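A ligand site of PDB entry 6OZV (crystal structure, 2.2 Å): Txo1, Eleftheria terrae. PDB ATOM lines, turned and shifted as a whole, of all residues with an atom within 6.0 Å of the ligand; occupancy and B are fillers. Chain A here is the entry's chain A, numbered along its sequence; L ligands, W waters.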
ATOM      1  N   THR A 617      -0.018  13.222  16.734  1.00  0.00           N
ATOM      2  CA  THR A 617       0.916  13.642  15.702  1.00  0.00           C
ATOM      3  C   THR A 617       1.947  12.539  15.490  1.00  0.00           C
ATOM      4  O   THR A 617       2.314  11.823  16.431  1.00  0.00           O
ATOM      5  CB  THR A 617       1.611  14.962  16.073  1.00  0.00           C
ATOM      6  OG1 THR A 617       2.375  15.424  14.965  1.00  0.00           O
ATOM      7  CG2 THR A 617       2.524  14.774  17.276  1.00  0.00           C
ATOM      8  N   PHE A 661      -6.087  16.619  11.908  1.00  0.00           N
ATOM      9  CA  PHE A 661      -5.099  17.690  11.905  1.00  0.00           C
ATOM     10  C   PHE A 661      -5.670  18.881  12.645  1.00  0.00           C
ATOM     11  O   PHE A 661      -6.828  19.259  12.433  1.00  0.00           O
ATOM     12  CB  PHE A 661      -4.723  18.076  10.474  1.00  0.00           C
ATOM     13  CG  PHE A 661      -4.076  16.972   9.690  1.00  0.00           C
ATOM     14  CD1 PHE A 661      -3.015  16.263  10.220  1.00  0.00           C
ATOM     15  CD2 PHE A 661      -4.527  16.643   8.419  1.00  0.00           C
ATOM     16  CE1 PHE A 661      -2.417  15.243   9.504  1.00  0.00           C
ATOM     17  CE2 PHE A 661      -3.928  15.623   7.703  1.00  0.00           C
ATOM     18  CZ  PHE A 661      -2.881  14.919   8.247  1.00  0.00           C
ATOM     19  N   ASP A 662      -4.859  19.493  13.522  1.00  0.00           N
ATOM     20  CA  ASP A 662      -5.409  20.497  14.415  1.00  0.00           C
ATOM     21  C   ASP A 662      -5.772  21.805  13.729  1.00  0.00           C
ATOM     22  O   ASP A 662      -6.384  22.669  14.371  1.00  0.00           O
ATOM     23  CB  ASP A 662      -4.434  20.772  15.574  1.00  0.00           C
ATOM     24  CG  ASP A 662      -3.146  21.439  15.128  1.00  0.00           C
ATOM     25  OD1 ASP A 662      -2.889  21.538  13.909  1.00  0.00           O
ATOM     26  OD2 ASP A 662      -2.378  21.859  16.017  1.00  0.00           O
ATOM     27  N   CYS A 731      -2.501  29.974   5.173  1.00  0.00           N
ATOM     28  CA  CYS A 731      -1.512  28.998   4.738  1.00  0.00           C
ATOM     29  C   CYS A 731      -0.665  28.586   5.940  1.00  0.00           C
ATOM     30  O   CYS A 731      -0.188  29.442   6.689  1.00  0.00           O
ATOM     31  CB  CYS A 731      -0.639  29.580   3.634  1.00  0.00           C
ATOM     32  SG  CYS A 731      -0.009  28.346   2.498  1.00  0.00           S
ATOM     33  N   SER A 732      -0.478  27.278   6.108  1.00  0.00           N
ATOM     34  CA  SER A 732       0.322  26.759   7.218  1.00  0.00           C
ATOM     35  C   SER A 732       0.757  25.340   6.895  1.00  0.00           C
ATOM     36  O   SER A 732       0.298  24.741   5.920  1.00  0.00           O
ATOM     37  CB  SER A 732      -0.461  26.794   8.535  1.00  0.00           C
ATOM     38  OG  SER A 732      -1.511  25.857   8.520  1.00  0.00           O
ATOM     39  N   GLY A 733       1.652  24.820   7.728  1.00  0.00           N
ATOM     40  CA  GLY A 733       2.062  23.426   7.597  1.00  0.00           C
ATOM     41  C   GLY A 733       3.412  23.222   6.955  1.00  0.00           C
ATOM     42  O   GLY A 733       4.232  22.446   7.452  1.00  0.00           O
ATOM     43  N   GLU A 734       3.653  23.911   5.831  1.00  0.00           N
ATOM     44  CA  GLU A 734       4.918  23.839   5.121  1.00  0.00           C
ATOM     45  C   GLU A 734       5.440  25.254   4.903  1.00  0.00           C
ATOM     46  O   GLU A 734       4.744  26.247   5.169  1.00  0.00           O
ATOM     47  CB  GLU A 734       4.762  23.134   3.760  1.00  0.00           C
ATOM     48  CG  GLU A 734       3.977  21.826   3.781  1.00  0.00           C
ATOM     49  CD  GLU A 734       3.413  21.447   2.420  1.00  0.00           C
ATOM     50  OE1 GLU A 734       3.452  22.274   1.483  1.00  0.00           O
ATOM     51  OE2 GLU A 734       2.918  20.303   2.274  1.00  0.00           O
ATOM     52  N   ALA A 735       6.670  25.351   4.412  1.00  0.00           N
ATOM     53  CA  ALA A 735       7.220  26.650   4.048  1.00  0.00           C
ATOM     54  C   ALA A 735       6.443  27.221   2.871  1.00  0.00           C
ATOM     55  O   ALA A 735       6.225  26.537   1.868  1.00  0.00           O
ATOM     56  CB  ALA A 735       8.701  26.511   3.704  1.00  0.00           C
ATOM     57  N   LEU A 736       6.031  28.481   3.002  1.00  0.00           N
ATOM     58  CA  LEU A 736       5.286  29.144   1.936  1.00  0.00           C
ATOM     59  C   LEU A 736       6.255  29.875   1.014  1.00  0.00           C
ATOM     60  O   LEU A 736       6.808  30.908   1.407  1.00  0.00           O
ATOM     61  CB  LEU A 736       4.283  30.132   2.524  1.00  0.00           C
ATOM     62  CG  LEU A 736       3.539  31.052   1.556  1.00  0.00           C
ATOM     63  CD1 LEU A 736       2.862  30.255   0.458  1.00  0.00           C
ATOM     64  CD2 LEU A 736       2.524  31.890   2.311  1.00  0.00           C
ATOM     65  N   ASN A 755       0.272  33.757   6.258  1.00  0.00           N
ATOM     66  CA  ASN A 755       1.157  32.629   6.554  1.00  0.00           C
ATOM     67  C   ASN A 755       1.172  32.415   8.054  1.00  0.00           C
ATOM     68  O   ASN A 755       1.608  33.288   8.814  1.00  0.00           O
ATOM     69  CB  ASN A 755       2.562  32.902   6.027  1.00  0.00           C
ATOM     70  CG  ASN A 755       3.453  31.677   6.092  1.00  0.00           C
ATOM     71  OD1 ASN A 755       2.975  30.547   6.001  1.00  0.00           O
ATOM     72  ND2 ASN A 755       4.752  31.895   6.233  1.00  0.00           N
ATOM     73  N   LEU A 756       0.691  31.247   8.494  1.00  0.00           N
ATOM     74  CA  LEU A 756       0.638  30.921   9.911  1.00  0.00           C
ATOM     75  C   LEU A 756       1.571  29.758  10.207  1.00  0.00           C
ATOM     76  O   LEU A 756       1.748  28.859   9.380  1.00  0.00           O
ATOM     77  CB  LEU A 756      -0.798  30.563  10.354  1.00  0.00           C
ATOM     78  CG  LEU A 756      -1.664  31.739  10.822  1.00  0.00           C
ATOM     79  CD1 LEU A 756      -1.865  32.773   9.717  1.00  0.00           C
ATOM     80  CD2 LEU A 756      -3.007  31.251  11.340  1.00  0.00           C
ATOM     81  N   TYR A 757       2.181  29.792  11.389  1.00  0.00           N
ATOM     82  CA  TYR A 757       3.143  28.776  11.804  1.00  0.00           C
ATOM     83  C   TYR A 757       2.801  28.295  13.200  1.00  0.00           C
ATOM     84  O   TYR A 757       2.411  29.083  14.063  1.00  0.00           O
ATOM     85  CB  TYR A 757       4.580  29.313  11.781  1.00  0.00           C
ATOM     86  CG  TYR A 757       5.554  28.508  12.615  1.00  0.00           C
ATOM     87  CD1 TYR A 757       6.203  27.403  12.089  1.00  0.00           C
ATOM     88  CD2 TYR A 757       5.810  28.863  13.935  1.00  0.00           C
ATOM     89  CE1 TYR A 757       7.080  26.661  12.867  1.00  0.00           C
ATOM     90  CE2 TYR A 757       6.687  28.130  14.710  1.00  0.00           C
ATOM     91  CZ  TYR A 757       7.315  27.035  14.175  1.00  0.00           C
ATOM     92  OH  TYR A 757       8.187  26.314  14.954  1.00  0.00           O
ATOM     93  N   GLY A 758       2.983  26.996  13.432  1.00  0.00           N
ATOM     94  CA  GLY A 758       2.838  26.441  14.756  1.00  0.00           C
ATOM     95  C   GLY A 758       2.747  24.934  14.745  1.00  0.00           C
ATOM     96  O   GLY A 758       2.196  24.313  13.819  1.00  0.00           O
ATOM     97  N   PRO A 759       3.301  24.305  15.776  1.00  0.00           N
ATOM     98  CA  PRO A 759       3.130  22.856  15.953  1.00  0.00           C
ATOM     99  C   PRO A 759       1.867  22.534  16.743  1.00  0.00           C
ATOM    100  O   PRO A 759       1.261  23.390  17.395  1.00  0.00           O
ATOM    101  CB  PRO A 759       4.381  22.470  16.749  1.00  0.00           C
ATOM    102  CG  PRO A 759       4.646  23.678  17.589  1.00  0.00           C
ATOM    103  CD  PRO A 759       4.234  24.874  16.753  1.00  0.00           C
ATOM    104  N   THR A 760       1.471  21.257  16.665  1.00  0.00           N
ATOM    105  CA  THR A 760       0.331  20.786  17.438  1.00  0.00           C
ATOM    106  C   THR A 760       0.541  21.005  18.930  1.00  0.00           C
ATOM    107  O   THR A 760      -0.407  21.331  19.654  1.00  0.00           O
ATOM    108  CB  THR A 760       0.081  19.304  17.143  1.00  0.00           C
ATOM    109  OG1 THR A 760      -0.096  19.106  15.732  1.00  0.00           O
ATOM    110  CG2 THR A 760      -1.162  18.797  17.873  1.00  0.00           C
ATOM    111  N   GLU A 761       1.785  20.873  19.406  1.00  0.00           N
ATOM    112  CA  GLU A 761       2.108  21.040  20.811  1.00  0.00           C
ATOM    113  C   GLU A 761       1.971  22.469  21.312  1.00  0.00           C
ATOM    114  O   GLU A 761       2.214  22.715  22.501  1.00  0.00           O
ATOM    115  CB  GLU A 761       3.528  20.534  21.072  1.00  0.00           C
ATOM    116  CG  GLU A 761       3.700  19.034  20.882  1.00  0.00           C
ATOM    117  CD  GLU A 761       4.018  18.633  19.453  1.00  0.00           C
ATOM    118  OE1 GLU A 761       4.575  17.534  19.261  1.00  0.00           O
ATOM    119  OE2 GLU A 761       3.719  19.407  18.513  1.00  0.00           O
ATOM    120  N   VAL A 764      -2.176  24.670  17.437  1.00  0.00           N
ATOM    121  CA  VAL A 764      -2.442  25.000  16.031  1.00  0.00           C
ATOM    122  C   VAL A 764      -1.399  25.961  15.467  1.00  0.00           C
ATOM    123  O   VAL A 764      -0.516  25.554  14.696  1.00  0.00           O
ATOM    124  CB  VAL A 764      -3.862  25.565  15.835  1.00  0.00           C
ATOM    125  CG1 VAL A 764      -4.169  25.751  14.354  1.00  0.00           C
ATOM    126  CG2 VAL A 764      -4.891  24.646  16.482  1.00  0.00           C
ATOM    127  N   ASP A 765      -1.474  27.242  15.822  1.00  0.00           N
ATOM    128  CA  ASP A 765      -0.562  28.242  15.291  1.00  0.00           C
ATOM    129  C   ASP A 765      -0.149  29.219  16.377  1.00  0.00           C
ATOM    130  O   ASP A 765      -0.920  29.523  17.287  1.00  0.00           O
ATOM    131  CB  ASP A 765      -1.205  28.995  14.121  1.00  0.00           C
ATOM    132  CG  ASP A 765      -1.496  28.098  12.939  1.00  0.00           C
ATOM    133  OD1 ASP A 765      -0.540  27.501  12.401  1.00  0.00           O
ATOM    134  OD2 ASP A 765      -2.677  27.974  12.567  1.00  0.00           O
ATOM    135  N   ILE A 782       7.379  33.781   8.830  1.00  0.00           N
ATOM    136  CA  ILE A 782       6.267  33.216   9.605  1.00  0.00           C
ATOM    137  C   ILE A 782       5.642  34.250  10.517  1.00  0.00           C
ATOM    138  O   ILE A 782       4.574  33.989  11.087  1.00  0.00           O
ATOM    139  CB  ILE A 782       6.698  31.990  10.412  1.00  0.00           C
ATOM    140  CG1 ILE A 782       7.840  32.341  11.363  1.00  0.00           C
ATOM    141  CG2 ILE A 782       7.101  30.850   9.484  1.00  0.00           C
ATOM    142  CD1 ILE A 782       8.271  31.178  12.248  1.00  0.00           C
ATOM    143  N   THR A 847      10.675  23.212  19.657  1.00  0.00           N
ATOM    144  CA  THR A 847      10.008  22.822  18.416  1.00  0.00           C
ATOM    145  C   THR A 847      10.849  21.893  17.557  1.00  0.00           C
ATOM    146  O   THR A 847      10.291  21.096  16.783  1.00  0.00           O
ATOM    147  CB  THR A 847       9.664  24.071  17.597  1.00  0.00           C
ATOM    148  OG1 THR A 847      10.881  24.713  17.192  1.00  0.00           O
ATOM    149  CG2 THR A 847       8.839  25.034  18.431  1.00  0.00           C
ATOM    150  N   ASP A 849      12.437  23.196  15.255  1.00  0.00           N
ATOM    151  CA  ASP A 849      12.497  24.046  14.075  1.00  0.00           C
ATOM    152  C   ASP A 849      13.641  25.044  14.215  1.00  0.00           C
ATOM    153  O   ASP A 849      13.893  25.563  15.305  1.00  0.00           O
ATOM    154  CB  ASP A 849      11.182  24.791  13.874  1.00  0.00           C
ATOM    155  CG  ASP A 849      10.035  23.864  13.539  1.00  0.00           C
ATOM    156  OD1 ASP A 849      10.238  22.891  12.789  1.00  0.00           O
ATOM    157  OD2 ASP A 849       8.910  24.116  14.036  1.00  0.00           O
ATOM    158  N   TYR A 861      11.294  31.104   9.147  1.00  0.00           N
ATOM    159  CA  TYR A 861      11.526  29.662   9.290  1.00  0.00           C
ATOM    160  C   TYR A 861      12.649  29.235   8.356  1.00  0.00           C
ATOM    161  O   TYR A 861      12.640  29.546   7.168  1.00  0.00           O
ATOM    162  CB  TYR A 861      10.243  28.888   8.987  1.00  0.00           C
ATOM    163  CG  TYR A 861      10.427  27.390   8.920  1.00  0.00           C
ATOM    164  CD1 TYR A 861      10.407  26.612  10.071  1.00  0.00           C
ATOM    165  CD2 TYR A 861      10.616  26.755   7.703  1.00  0.00           C
ATOM    166  CE1 TYR A 861      10.572  25.229  10.004  1.00  0.00           C
ATOM    167  CE2 TYR A 861      10.780  25.379   7.620  1.00  0.00           C
ATOM    168  CZ  TYR A 861      10.748  24.624   8.779  1.00  0.00           C
ATOM    169  OH  TYR A 861      10.913  23.257   8.692  1.00  0.00           O
ATOM    170  N   ARG A 864      14.471  22.329   9.633  1.00  0.00           N
ATOM    171  CA  ARG A 864      14.475  21.472  10.804  1.00  0.00           C
ATOM    172  C   ARG A 864      15.880  21.355  11.369  1.00  0.00           C
ATOM    173  O   ARG A 864      16.870  21.410  10.641  1.00  0.00           O
ATOM    174  CB  ARG A 864      13.939  20.074  10.452  1.00  0.00           C
ATOM    175  CG  ARG A 864      12.468  20.065  10.051  1.00  0.00           C
ATOM    176  CD  ARG A 864      11.576  20.332  11.243  1.00  0.00           C
ATOM    177  NE  ARG A 864      11.695  19.289  12.260  1.00  0.00           N
ATOM    178  CZ  ARG A 864      11.136  19.338  13.456  1.00  0.00           C
ATOM    179  NH1 ARG A 864      10.412  20.390  13.818  1.00  0.00           N
ATOM    180  NH2 ARG A 864      11.302  18.341  14.318  1.00  0.00           N
HETATM  181  P1  LIG L   1       2.041  19.764  12.892  1.00  0.00           P
HETATM  182  O1  LIG L   1       0.948  20.759  12.630  1.00  0.00           O
HETATM  183  O2  LIG L   1       2.468  19.676  14.339  1.00  0.00           O
HETATM  184  O3  LIG L   1       1.872  18.414  12.233  1.00  0.00           O
HETATM  185  O4  LIG L   1       3.280  20.420  12.136  1.00  0.00           O
HETATM  186  C1  LIG L   1       4.154  21.307  12.822  1.00  0.00           C
HETATM  187  C2  LIG L   1       5.399  21.585  12.016  1.00  0.00           C
HETATM  188  O5  LIG L   1       5.056  21.978  10.671  1.00  0.00           O
HETATM  189  C3  LIG L   1       6.256  22.732  12.514  1.00  0.00           C
HETATM  190  O6  LIG L   1       7.069  22.388  13.619  1.00  0.00           O
HETATM  191  C4  LIG L   1       7.038  23.126  11.277  1.00  0.00           C
HETATM  192  O7  LIG L   1       8.127  22.227  11.064  1.00  0.00           O
HETATM  193  C5  LIG L   1       6.005  22.892  10.177  1.00  0.00           C
HETATM  194  N1  LIG L   1       5.304  24.140   9.829  1.00  0.00           N
HETATM  195  C6  LIG L   1       4.087  24.527  10.265  1.00  0.00           C
HETATM  196  N2  LIG L   1       3.738  25.736   9.752  1.00  0.00           N
HETATM  197  C7  LIG L   1       4.752  26.149   8.966  1.00  0.00           C
HETATM  198  C8  LIG L   1       5.049  27.342   8.132  1.00  0.00           C
HETATM  199  N3  LIG L   1       4.155  28.356   8.022  1.00  0.00           N
HETATM  200  N4  LIG L   1       6.225  27.377   7.486  1.00  0.00           N
HETATM  201  C9  LIG L   1       7.120  26.378   7.577  1.00  0.00           C
HETATM  202  N5  LIG L   1       6.917  25.267   8.316  1.00  0.00           N
HETATM  203  C10 LIG L   1       5.783  25.099   9.019  1.00  0.00           C
HETATM  204  O   HOH W   1       6.654  19.937  14.728  1.00  0.00           O
HETATM  205  O   HOH W   2       2.593  27.874   5.141  1.00  0.00           O
HETATM  206  O   HOH W   3       3.776  17.865   9.897  1.00  0.00           O
HETATM  207  O   HOH W   4       0.347  16.569  12.844  1.00  0.00           O
HETATM  208  O   HOH W   5       2.512  19.979   9.136  1.00  0.00           O
HETATM  209  O   HOH W   6      -0.607  22.884  13.472  1.00  0.00           O
HETATM  210  O   HOH W   7       1.119  17.844   9.518  1.00  0.00           O
HETATM  211  O   HOH W   8       8.331  22.892   7.442  1.00  0.00           O
HETATM  212  O   HOH W   9      -1.663  19.911  11.545  1.00  0.00           O
HETATM  213  O   HOH W  10       6.533  29.459   5.780  1.00  0.00           O
HETATM  214  O   HOH W  11       1.235  22.893  10.661  1.00  0.00           O
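Water W4 lies within hydrogen-bond range of O3 of the ligand (2.5 Å) and OG1 of Thr 617 (3.1 Å).
Water W10 lies within hydrogen-bond range of a nitrogen (N4) of the ligand (2.7 Å), the backbone NH (N) of Leu 736 (3.0 Å) and the side-chain amide nitrogen (ND2) of Asn 755 (3.1 Å).
Water W8 lies within hydrogen-bond range of OH of Tyr 861 (2.9 Å) and N5 of the ligand (2.9 Å).
Water W9 bridges an oxygen (O1) of the ligand (3.0 Å) and the side-chain carboxylate of Asp 662 (3.1 Å).
Water W5 bridges an oxygen (O4) of the ligand and the backbone carbonyl oxygen of Gly 733.
Water W2 lies within hydrogen-bond range of O of Glu 734, OD1 of Asn 755, N of Ser 732, N3 of the ligand and SG of Cys 731.
The backbone NH (N) of Thr 760 sits at hydrogen-bond distance from an oxygen (O2) of the ligand.
An oxygen (O6) of the ligand lies within hydrogen-bond range of the side-chain carboxylate (OD2) of Asp 849, at 2.6 Å.
The side-chain amide oxygen (OD1) of Asn 755 is in hydrogen-bond range of a nitrogen (N3) of the ligand.
O2 of the ligand is in hydrogen-bond range of OG1 of Thr 760.
The backbone carbonyl oxygen (O) of Leu 756 lies within hydrogen-bond range of a nitrogen (N3) of the ligand (2.8 Å).
N of Gly 733 is in hydrogen-bond range of N2 of the ligand (3.0 Å).
OD1 of Asp 849 is in salt-bridge range of NH1 of Arg 864, 2.7 Å away.
The guanidinium group (NH1) of Arg 864 is in hydrogen-bond range of the backbone carbonyl oxygen (O) of Thr 847, 3.1 Å away.
The side-chain hydroxyl (OH) of Tyr 757 is in hydrogen-bond range of the side-chain carboxylate (OD2) of Asp 849 (2.5 Å).
The backbone NH (N) of Leu 756 is in hydrogen-bond range of the backbone carbonyl oxygen (O) of Cys 731 (2.7 Å).
The side-chain amide oxygen of Asn 755 lies close to the backbone carbonyl oxygen of Cys 731, at 3.4 Å.
The backbone NH of Asp 849 is in hydrogen-bond range of the side-chain hydroxyl of Thr 847 (2.9 Å).
O of Glu 734 sits close to N4 of the ligand (3.0 Å).
Merely in contact with the ligand: Ala 735, Tyr 861, Pro 759, Tyr 757, Gly 758 and Arg 864.
Hydrophobic or aromatic side chains that line the ligand: Tyr 757 and Tyr 861.
12 residues have an atom within 4 Å of the ligand: Gly 733, Glu 734, Ala 735, Asn 755, Leu 756, Tyr 757, Gly 758, Pro 759, Thr 760, Asp 849, Tyr 861 and Arg 864.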
